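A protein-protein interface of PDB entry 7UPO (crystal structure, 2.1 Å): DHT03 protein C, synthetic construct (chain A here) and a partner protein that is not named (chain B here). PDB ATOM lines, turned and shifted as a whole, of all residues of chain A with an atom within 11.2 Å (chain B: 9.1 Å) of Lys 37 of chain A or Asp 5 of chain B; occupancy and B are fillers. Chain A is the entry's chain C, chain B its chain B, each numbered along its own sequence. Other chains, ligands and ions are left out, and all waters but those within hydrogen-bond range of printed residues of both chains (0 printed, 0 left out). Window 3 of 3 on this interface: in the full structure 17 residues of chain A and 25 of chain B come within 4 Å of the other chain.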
ATOM      1  N   GLN A  28      21.172   6.807  22.641  1.00  0.00           N
ATOM      2  CA  GLN A  28      22.314   5.924  22.419  1.00  0.00           C
ATOM      3  C   GLN A  28      22.697   5.179  23.690  1.00  0.00           C
ATOM      4  O   GLN A  28      23.067   4.001  23.635  1.00  0.00           O
ATOM      5  CB  GLN A  28      23.506   6.719  21.893  1.00  0.00           C
ATOM      6  CG  GLN A  28      23.337   7.229  20.477  1.00  0.00           C
ATOM      7  CD  GLN A  28      24.651   7.666  19.863  1.00  0.00           C
ATOM      8  OE1 GLN A  28      25.721   7.210  20.267  1.00  0.00           O
ATOM      9  NE2 GLN A  28      24.577   8.558  18.881  1.00  0.00           N
ATOM     10  N   ILE A  29      22.621   5.846  24.843  1.00  0.00           N
ATOM     11  CA  ILE A  29      22.970   5.187  26.097  1.00  0.00           C
ATOM     12  C   ILE A  29      21.976   4.076  26.410  1.00  0.00           C
ATOM     13  O   ILE A  29      22.366   2.969  26.804  1.00  0.00           O
ATOM     14  CB  ILE A  29      23.053   6.214  27.241  1.00  0.00           C
ATOM     15  CG1 ILE A  29      24.190   7.205  26.990  1.00  0.00           C
ATOM     16  CG2 ILE A  29      23.258   5.511  28.569  1.00  0.00           C
ATOM     17  CD1 ILE A  29      24.308   8.275  28.053  1.00  0.00           C
ATOM     18  N   LYS A  30      20.681   4.347  26.236  1.00  0.00           N
ATOM     19  CA  LYS A  30      19.675   3.309  26.447  1.00  0.00           C
ATOM     20  C   LYS A  30      19.877   2.143  25.487  1.00  0.00           C
ATOM     21  O   LYS A  30      19.713   0.978  25.869  1.00  0.00           O
ATOM     22  CB  LYS A  30      18.273   3.889  26.279  1.00  0.00           C
ATOM     23  CG  LYS A  30      17.862   4.895  27.334  1.00  0.00           C
ATOM     24  CD  LYS A  30      16.473   5.430  27.025  1.00  0.00           C
ATOM     25  CE  LYS A  30      15.994   6.381  28.099  1.00  0.00           C
ATOM     26  NZ  LYS A  30      14.723   7.046  27.706  1.00  0.00           N
ATOM     27  N   LEU A  31      20.226   2.439  24.233  1.00  0.00           N
ATOM     28  CA  LEU A  31      20.428   1.378  23.253  1.00  0.00           C
ATOM     29  C   LEU A  31      21.613   0.498  23.628  1.00  0.00           C
ATOM     30  O   LEU A  31      21.559  -0.729  23.473  1.00  0.00           O
ATOM     31  CB  LEU A  31      20.620   1.980  21.862  1.00  0.00           C
ATOM     32  CG  LEU A  31      19.368   2.603  21.242  1.00  0.00           C
ATOM     33  CD1 LEU A  31      19.663   3.212  19.880  1.00  0.00           C
ATOM     34  CD2 LEU A  31      18.271   1.563  21.144  1.00  0.00           C
ATOM     35  N   PHE A  32      22.693   1.103  24.127  1.00  0.00           N
ATOM     36  CA  PHE A  32      23.842   0.310  24.548  1.00  0.00           C
ATOM     37  C   PHE A  32      23.541  -0.495  25.804  1.00  0.00           C
ATOM     38  O   PHE A  32      24.045  -1.612  25.953  1.00  0.00           O
ATOM     39  CB  PHE A  32      25.059   1.208  24.769  1.00  0.00           C
ATOM     40  CG  PHE A  32      25.819   1.513  23.511  1.00  0.00           C
ATOM     41  CD1 PHE A  32      26.438   0.496  22.803  1.00  0.00           C
ATOM     42  CD2 PHE A  32      25.925   2.811  23.040  1.00  0.00           C
ATOM     43  CE1 PHE A  32      27.141   0.766  21.643  1.00  0.00           C
ATOM     44  CE2 PHE A  32      26.627   3.087  21.881  1.00  0.00           C
ATOM     45  CZ  PHE A  32      27.236   2.065  21.183  1.00  0.00           C
ATOM     46  N   ILE A  33      22.727   0.050  26.713  1.00  0.00           N
ATOM     47  CA  ILE A  33      22.328  -0.703  27.900  1.00  0.00           C
ATOM     48  C   ILE A  33      21.659  -2.010  27.495  1.00  0.00           C
ATOM     49  O   ILE A  33      21.936  -3.072  28.066  1.00  0.00           O
ATOM     50  CB  ILE A  33      21.410   0.150  28.796  1.00  0.00           C
ATOM     51  CG1 ILE A  33      22.196   1.297  29.435  1.00  0.00           C
ATOM     52  CG2 ILE A  33      20.758  -0.711  29.872  1.00  0.00           C
ATOM     53  CD1 ILE A  33      21.323   2.303  30.164  1.00  0.00           C
ATOM     54  N   GLU A  34      20.783  -1.957  26.490  1.00  0.00           N
ATOM     55  CA  GLU A  34      20.119  -3.170  26.030  1.00  0.00           C
ATOM     56  C   GLU A  34      21.036  -4.029  25.166  1.00  0.00           C
ATOM     57  O   GLU A  34      20.948  -5.261  25.218  1.00  0.00           O
ATOM     58  CB  GLU A  34      18.843  -2.812  25.265  1.00  0.00           C
ATOM     59  CG  GLU A  34      17.946  -4.004  24.952  1.00  0.00           C
ATOM     60  CD  GLU A  34      17.404  -4.680  26.194  1.00  0.00           C
ATOM     61  OE1 GLU A  34      17.039  -3.965  27.152  1.00  0.00           O
ATOM     62  OE2 GLU A  34      17.345  -5.929  26.213  1.00  0.00           O
ATOM     63  N   LEU A  35      21.921  -3.407  24.380  1.00  0.00           N
ATOM     64  CA  LEU A  35      22.864  -4.175  23.570  1.00  0.00           C
ATOM     65  C   LEU A  35      23.846  -4.947  24.443  1.00  0.00           C
ATOM     66  O   LEU A  35      24.217  -6.080  24.117  1.00  0.00           O
ATOM     67  CB  LEU A  35      23.617  -3.247  22.618  1.00  0.00           C
ATOM     68  CG  LEU A  35      22.932  -2.892  21.299  1.00  0.00           C
ATOM     69  CD1 LEU A  35      23.726  -1.830  20.557  1.00  0.00           C
ATOM     70  CD2 LEU A  35      22.769  -4.135  20.441  1.00  0.00           C
ATOM     71  N   ILE A  36      24.288  -4.344  25.548  1.00  0.00           N
ATOM     72  CA  ILE A  36      25.185  -5.035  26.467  1.00  0.00           C
ATOM     73  C   ILE A  36      24.458  -6.181  27.158  1.00  0.00           C
ATOM     74  O   ILE A  36      25.026  -7.260  27.369  1.00  0.00           O
ATOM     75  CB  ILE A  36      25.777  -4.036  27.477  1.00  0.00           C
ATOM     76  CG1 ILE A  36      26.705  -3.051  26.762  1.00  0.00           C
ATOM     77  CG2 ILE A  36      26.523  -4.762  28.585  1.00  0.00           C
ATOM     78  CD1 ILE A  36      26.874  -1.732  27.484  1.00  0.00           C
ATOM     79  N   LYS A  37      23.187  -5.973  27.513  1.00  0.00           N
ATOM     80  CA  LYS A  37      22.407  -7.048  28.116  1.00  0.00           C
ATOM     81  C   LYS A  37      22.034  -8.106  27.084  1.00  0.00           C
ATOM     82  O   LYS A  37      22.029  -9.304  27.390  1.00  0.00           O
ATOM     83  CB  LYS A  37      21.157  -6.478  28.784  1.00  0.00           C
ATOM     84  CG  LYS A  37      21.448  -5.621  30.006  1.00  0.00           C
ATOM     85  CD  LYS A  37      20.180  -5.005  30.575  1.00  0.00           C
ATOM     86  CE  LYS A  37      20.485  -4.134  31.783  1.00  0.00           C
ATOM     87  NZ  LYS A  37      19.294  -3.358  32.232  1.00  0.00           N
ATOM     88  N   ARG A  38      21.725  -7.688  25.856  1.00  0.00           N
ATOM     89  CA  ARG A  38      21.390  -8.633  24.797  1.00  0.00           C
ATOM     90  C   ARG A  38      21.658  -8.029  23.423  1.00  0.00           C
ATOM     91  O   ARG A  38      21.065  -7.003  23.067  1.00  0.00           O
ATOM     92  CB  ARG A  38      19.928  -9.068  24.904  1.00  0.00           C
ATOM     93  CG  ARG A  38      19.514 -10.059  23.831  1.00  0.00           C
ATOM     94  CD  ARG A  38      18.126 -10.615  24.086  1.00  0.00           C
ATOM     95  NE  ARG A  38      17.794 -11.673  23.137  1.00  0.00           N
ATOM     96  CZ  ARG A  38      18.140 -12.947  23.286  1.00  0.00           C
ATOM     97  NH1 ARG A  38      18.834 -13.329  24.351  1.00  0.00           N
ATOM     98  NH2 ARG A  38      17.796 -13.841  22.372  1.00  0.00           N
ATOM     99  N   PRO A  39      22.539  -8.632  22.626  1.00  0.00           N
ATOM    100  CA  PRO A  39      22.808  -8.097  21.286  1.00  0.00           C
ATOM    101  C   PRO A  39      21.597  -8.238  20.376  1.00  0.00           C
ATOM    102  O   PRO A  39      20.885  -9.244  20.405  1.00  0.00           O
ATOM    103  CB  PRO A  39      23.982  -8.949  20.788  1.00  0.00           C
ATOM    104  CG  PRO A  39      24.576  -9.557  22.023  1.00  0.00           C
ATOM    105  CD  PRO A  39      23.426  -9.758  22.958  1.00  0.00           C
ATOM    106  N   ASP A  40      21.373  -7.211  19.560  1.00  0.00           N
ATOM    107  CA  ASP A  40      20.270  -7.200  18.607  1.00  0.00           C
ATOM    108  C   ASP A  40      20.652  -6.294  17.447  1.00  0.00           C
ATOM    109  O   ASP A  40      21.080  -5.156  17.666  1.00  0.00           O
ATOM    110  CB  ASP A  40      18.973  -6.716  19.266  1.00  0.00           C
ATOM    111  CG  ASP A  40      17.776  -6.802  18.338  1.00  0.00           C
ATOM    112  OD1 ASP A  40      17.857  -7.517  17.318  1.00  0.00           O
ATOM    113  OD2 ASP A  40      16.752  -6.149  18.629  1.00  0.00           O
ATOM    114  N   GLU A  41      20.496  -6.800  16.222  1.00  0.00           N
ATOM    115  CA  GLU A  41      20.916  -6.033  15.054  1.00  0.00           C
ATOM    116  C   GLU A  41      20.026  -4.816  14.836  1.00  0.00           C
ATOM    117  O   GLU A  41      20.506  -3.759  14.409  1.00  0.00           O
ATOM    118  CB  GLU A  41      20.925  -6.924  13.812  1.00  0.00           C
ATOM    119  CG  GLU A  41      21.632  -6.305  12.620  1.00  0.00           C
ATOM    120  CD  GLU A  41      23.095  -6.018  12.899  1.00  0.00           C
ATOM    121  OE1 GLU A  41      23.726  -6.801  13.641  1.00  0.00           O
ATOM    122  OE2 GLU A  41      23.614  -5.006  12.380  1.00  0.00           O
ATOM    123  N   LEU A  43      18.683  -3.082  17.192  1.00  0.00           N
ATOM    124  CA  LEU A  43      19.196  -2.097  18.136  1.00  0.00           C
ATOM    125  C   LEU A  43      20.492  -1.479  17.630  1.00  0.00           C
ATOM    126  O   LEU A  43      20.698  -0.269  17.757  1.00  0.00           O
ATOM    127  CB  LEU A  43      19.409  -2.737  19.505  1.00  0.00           C
ATOM    128  CG  LEU A  43      18.153  -3.222  20.225  1.00  0.00           C
ATOM    129  CD1 LEU A  43      18.544  -3.923  21.509  1.00  0.00           C
ATOM    130  CD2 LEU A  43      17.206  -2.063  20.505  1.00  0.00           C
ATOM    131  N   SER B   1      22.220  -2.150  42.947  1.00  0.00           N
ATOM    132  CA  SER B   1      23.063  -3.320  43.157  1.00  0.00           C
ATOM    133  C   SER B   1      23.893  -3.630  41.913  1.00  0.00           C
ATOM    134  O   SER B   1      25.120  -3.537  41.937  1.00  0.00           O
ATOM    135  CB  SER B   1      22.213  -4.535  43.537  1.00  0.00           C
ATOM    136  OG  SER B   1      23.020  -5.684  43.734  1.00  0.00           O
ATOM    137  N   SER B   2      23.213  -3.995  40.830  1.00  0.00           N
ATOM    138  CA  SER B   2      23.909  -4.322  39.595  1.00  0.00           C
ATOM    139  C   SER B   2      24.504  -3.058  38.975  1.00  0.00           C
ATOM    140  O   SER B   2      23.855  -2.008  38.963  1.00  0.00           O
ATOM    141  CB  SER B   2      22.957  -4.995  38.606  1.00  0.00           C
ATOM    142  OG  SER B   2      23.618  -5.322  37.396  1.00  0.00           O
ATOM    143  N   PRO B   3      25.730  -3.130  38.447  1.00  0.00           N
ATOM    144  CA  PRO B   3      26.374  -1.901  37.948  1.00  0.00           C
ATOM    145  C   PRO B   3      25.694  -1.315  36.724  1.00  0.00           C
ATOM    146  O   PRO B   3      25.565  -0.087  36.626  1.00  0.00           O
ATOM    147  CB  PRO B   3      27.805  -2.363  37.645  1.00  0.00           C
ATOM    148  CG  PRO B   3      27.674  -3.826  37.369  1.00  0.00           C
ATOM    149  CD  PRO B   3      26.587  -4.317  38.282  1.00  0.00           C
ATOM    150  N   VAL B   4      25.264  -2.153  35.778  1.00  0.00           N
ATOM    151  CA  VAL B   4      24.555  -1.643  34.608  1.00  0.00           C
ATOM    152  C   VAL B   4      23.188  -1.105  35.011  1.00  0.00           C
ATOM    153  O   VAL B   4      22.718  -0.095  34.472  1.00  0.00           O
ATOM    154  CB  VAL B   4      24.442  -2.738  33.530  1.00  0.00           C
ATOM    155  CG1 VAL B   4      23.769  -2.191  32.279  1.00  0.00           C
ATOM    156  CG2 VAL B   4      25.815  -3.296  33.196  1.00  0.00           C
ATOM    157  N   ASP B   5      22.533  -1.761  35.972  1.00  0.00           N
ATOM    158  CA  ASP B   5      21.240  -1.282  36.444  1.00  0.00           C
ATOM    159  C   ASP B   5      21.376   0.018  37.228  1.00  0.00           C
ATOM    160  O   ASP B   5      20.455   0.844  37.217  1.00  0.00           O
ATOM    161  CB  ASP B   5      20.563  -2.358  37.292  1.00  0.00           C
ATOM    162  CG  ASP B   5      20.245  -3.610  36.495  1.00  0.00           C
ATOM    163  OD1 ASP B   5      20.053  -3.499  35.266  1.00  0.00           O
ATOM    164  OD2 ASP B   5      20.186  -4.704  37.094  1.00  0.00           O
ATOM    165  N   GLU B   6      22.506   0.217  37.915  1.00  0.00           N
ATOM    166  CA  GLU B   6      22.764   1.505  38.552  1.00  0.00           C
ATOM    167  C   GLU B   6      22.909   2.606  37.511  1.00  0.00           C
ATOM    168  O   GLU B   6      22.453   3.736  37.723  1.00  0.00           O
ATOM    169  CB  GLU B   6      24.019   1.424  39.422  1.00  0.00           C
ATOM    170  CG  GLU B   6      23.857   0.619  40.707  1.00  0.00           C
ATOM    171  CD  GLU B   6      23.275   1.439  41.845  1.00  0.00           C
ATOM    172  OE1 GLU B   6      22.815   2.573  41.593  1.00  0.00           O
ATOM    173  OE2 GLU B   6      23.285   0.950  42.995  1.00  0.00           O
ATOM    174  N   ILE B   7      23.544   2.295  36.380  1.00  0.00           N
ATOM    175  CA  ILE B   7      23.677   3.275  35.308  1.00  0.00           C
ATOM    176  C   ILE B   7      22.327   3.543  34.661  1.00  0.00           C
ATOM    177  O   ILE B   7      21.982   4.695  34.367  1.00  0.00           O
ATOM    178  CB  ILE B   7      24.723   2.798  34.285  1.00  0.00           C
ATOM    179  CG1 ILE B   7      26.121   2.912  34.891  1.00  0.00           C
ATOM    180  CG2 ILE B   7      24.616   3.590  32.990  1.00  0.00           C
ATOM    181  CD1 ILE B   7      27.225   2.783  33.893  1.00  0.00           C
ATOM    182  N   ASP B   8      21.538   2.489  34.436  1.00  0.00           N
ATOM    183  CA  ASP B   8      20.175   2.670  33.948  1.00  0.00           C
ATOM    184  C   ASP B   8      19.393   3.604  34.864  1.00  0.00           C
ATOM    185  O   ASP B   8      18.683   4.501  34.394  1.00  0.00           O
ATOM    186  CB  ASP B   8      19.481   1.311  33.838  1.00  0.00           C
ATOM    187  CG  ASP B   8      18.244   1.352  32.962  1.00  0.00           C
ATOM    188  OD1 ASP B   8      17.890   2.444  32.470  1.00  0.00           O
ATOM    189  OD2 ASP B   8      17.628   0.283  32.760  1.00  0.00           O
ATOM    190  N   LYS B   9      19.534   3.417  36.180  1.00  0.00           N
ATOM    191  CA  LYS B   9      18.888   4.305  37.141  1.00  0.00           C
ATOM    192  C   LYS B   9      19.391   5.736  36.994  1.00  0.00           C
ATOM    193  O   LYS B   9      18.604   6.689  37.049  1.00  0.00           O
ATOM    194  CB  LYS B   9      19.135   3.793  38.561  1.00  0.00           C
ATOM    195  CG  LYS B   9      18.577   4.672  39.674  1.00  0.00           C
ATOM    196  CD  LYS B   9      17.089   4.437  39.883  1.00  0.00           C
ATOM    197  CE  LYS B   9      16.603   5.091  41.170  1.00  0.00           C
ATOM    198  NZ  LYS B   9      16.798   6.567  41.163  1.00  0.00           N
ATOM    199  N   GLU B  10      20.700   5.908  36.804  1.00  0.00           N
ATOM    200  CA  GLU B  10      21.256   7.253  36.707  1.00  0.00           C
ATOM    201  C   GLU B  10      20.828   7.950  35.421  1.00  0.00           C
ATOM    202  O   GLU B  10      20.634   9.171  35.418  1.00  0.00           O
ATOM    203  CB  GLU B  10      22.781   7.198  36.809  1.00  0.00           C
ATOM    204  CG  GLU B  10      23.444   8.561  36.928  1.00  0.00           C
ATOM    205  CD  GLU B  10      23.080   9.287  38.208  1.00  0.00           C
ATOM    206  OE1 GLU B  10      22.784   8.611  39.217  1.00  0.00           O
ATOM    207  OE2 GLU B  10      23.087  10.536  38.206  1.00  0.00           O
ATOM    208  N   VAL B  11      20.669   7.199  34.328  1.00  0.00           N
ATOM    209  CA  VAL B  11      20.234   7.804  33.072  1.00  0.00           C
ATOM    210  C   VAL B  11      18.801   8.304  33.188  1.00  0.00           C
ATOM    211  O   VAL B  11      18.462   9.381  32.684  1.00  0.00           O
ATOM    212  CB  VAL B  11      20.395   6.804  31.913  1.00  0.00           C
ATOM    213  CG1 VAL B  11      19.815   7.377  30.629  1.00  0.00           C
ATOM    214  CG2 VAL B  11      21.857   6.458  31.722  1.00  0.00           C
ATOM    215  N   LYS B  12      17.936   7.534  33.853  1.00  0.00           N
ATOM    216  CA  LYS B  12      16.558   7.969  34.049  1.00  0.00           C
ATOM    217  C   LYS B  12      16.498   9.247  34.877  1.00  0.00           C
ATOM    218  O   LYS B  12      15.635  10.103  34.652  1.00  0.00           O
ATOM    219  CB  LYS B  12      15.746   6.857  34.714  1.00  0.00           C
ATOM    220  CG  LYS B  12      15.658   5.573  33.900  1.00  0.00           C
ATOM    221  CD  LYS B  12      14.874   5.778  32.611  1.00  0.00           C
ATOM    222  CE  LYS B  12      14.749   4.479  31.824  1.00  0.00           C
ATOM    223  NZ  LYS B  12      16.071   3.959  31.376  1.00  0.00           N
ATOM    224  N   ARG B  72      31.141   5.652  32.175  1.00  0.00           N
ATOM    225  CA  ARG B  72      31.040   4.554  33.131  1.00  0.00           C
ATOM    226  C   ARG B  72      30.443   3.314  32.479  1.00  0.00           C
ATOM    227  O   ARG B  72      30.838   2.185  32.797  1.00  0.00           O
ATOM    228  CB  ARG B  72      30.203   4.984  34.335  1.00  0.00           C
ATOM    229  CG  ARG B  72      30.893   5.981  35.248  1.00  0.00           C
ATOM    230  CD  ARG B  72      29.879   6.738  36.089  1.00  0.00           C
ATOM    231  NE  ARG B  72      28.918   5.842  36.727  1.00  0.00           N
ATOM    232  CZ  ARG B  72      27.827   6.253  37.366  1.00  0.00           C
ATOM    233  NH1 ARG B  72      27.556   7.547  37.453  1.00  0.00           N
ATOM    234  NH2 ARG B  72      27.005   5.367  37.918  1.00  0.00           N
ATOM    235  N   LEU B  73      29.496   3.503  31.558  1.00  0.00           N
ATOM    236  CA  LEU B  73      28.917   2.369  30.844  1.00  0.00           C
ATOM    237  C   LEU B  73      29.968   1.651  30.011  1.00  0.00           C
ATOM    238  O   LEU B  73      29.973   0.416  29.931  1.00  0.00           O
ATOM    239  CB  LEU B  73      27.765   2.841  29.959  1.00  0.00           C
ATOM    240  CG  LEU B  73      27.047   1.759  29.154  1.00  0.00           C
ATOM    241  CD1 LEU B  73      26.376   0.767  30.088  1.00  0.00           C
ATOM    242  CD2 LEU B  73      26.033   2.379  28.206  1.00  0.00           C
ATOM    243  N   ILE B  76      32.416  -0.403  32.236  1.00  0.00           N
ATOM    244  CA  ILE B  76      31.856  -1.605  32.848  1.00  0.00           C
ATOM    245  C   ILE B  76      32.144  -2.826  31.983  1.00  0.00           C
ATOM    246  O   ILE B  76      32.629  -3.853  32.472  1.00  0.00           O
ATOM    247  CB  ILE B  76      30.348  -1.432  33.095  1.00  0.00           C
ATOM    248  CG1 ILE B  76      30.104  -0.523  34.301  1.00  0.00           C
ATOM    249  CG2 ILE B  76      29.679  -2.783  33.296  1.00  0.00           C
ATOM    250  CD1 ILE B  76      28.650  -0.413  34.693  1.00  0.00           C
ATOM    251  N   ILE B  77      31.856  -2.731  30.683  1.00  0.00           N
ATOM    252  CA  ILE B  77      32.058  -3.861  29.783  1.00  0.00           C
ATOM    253  C   ILE B  77      33.524  -4.122  29.482  1.00  0.00           C
ATOM    254  O   ILE B  77      33.851  -5.151  28.881  1.00  0.00           O
ATOM    255  CB  ILE B  77      31.306  -3.653  28.455  1.00  0.00           C
ATOM    256  CG1 ILE B  77      32.096  -2.723  27.534  1.00  0.00           C
ATOM    257  CG2 ILE B  77      29.924  -3.089  28.723  1.00  0.00           C
ATOM    258  CD1 ILE B  77      31.638  -2.760  26.095  1.00  0.00           C
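Of chain B, only Val 4 (3.8 Å) and Asp 5 (3.1 Å) come within 4 Å of Lys 37 of chain A.
Asp 5 of chain B touches just one residue of chain A: Lys 37 (3.1 Å).
No residue of chain A comes within 4 Å of Ser 2 of chain B.
No residue of chain A comes within 4 Å of Pro 3 of chain B.
Of chain A, only Lys 37 comes within 4 Å of Val 4 of chain B.
No residue of chain A comes within 4 Å of Glu 6 of chain B.
Asp 8 of chain B touches just one residue of chain A: Ile 33 (3.97 Å).
Printed residues of chain B within 4 Å of Ile 33 of chain A: Asp 8.
Of the printed residues of chain A, Ile 77 of chain B touches Ile 36 (3.6 Å).
Lys 12 of chain B touches none of the printed residues of chain A.
Arg 72 of chain B touches none of the printed residues of chain A.
The nearest printed residue of chain B that does not touch Ile 36 of chain A is Val 4 of chain B (4.9 Å).
Among the printed residues, merely in contact across the chains: Ile 29 of chain A with Val 11 of chain B (3.6 Å), Ile 29 of chain A with Leu 73 of chain B (3.97 Å), Phe 32 of chain A with Leu 73 of chain B (3.8 Å), Ile 33 of chain A with Asp 8 of chain B (3.97 Å), Ile 36 of chain A with Leu 73 of chain B (3.6 Å), Ile 36 of chain A with Ile 77 of chain B (3.6 Å) and Lys 37 of chain A with Val 4 of chain B (3.8 Å).
Printed residues of chain A that touch a printed residue of chain B: Ile 29, Phe 32, Ile 33, Ile 36 and Lys 37.
Hydrophobic or aromatic side chains of chain A within 4 Å of the printed part of chain B: Ile 29, Phe 32, Ile 33 and Ile 36.
Of the 16 printed residues of chain B, 6 touch a printed residue of chain A.
Among the printed residues, Asp or Glu carboxylates within 4 Å of a Lys or Arg side-chain nitrogen of the other chain: Lys 37 of chain A with Asp 5 of chain B.
The side-chain carboxylate (OD1) of Asp 5 of chain B lies within salt-bridge range of the side-chain amino group (NZ) of Lys 37 of chain A, 3.1 Å away.
The side-chain carboxylate (OD1) of Asp 8 of chain B lies within salt-bridge range of the side-chain amino group (NZ) of Lys 12 of chain B (2.6 Å).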
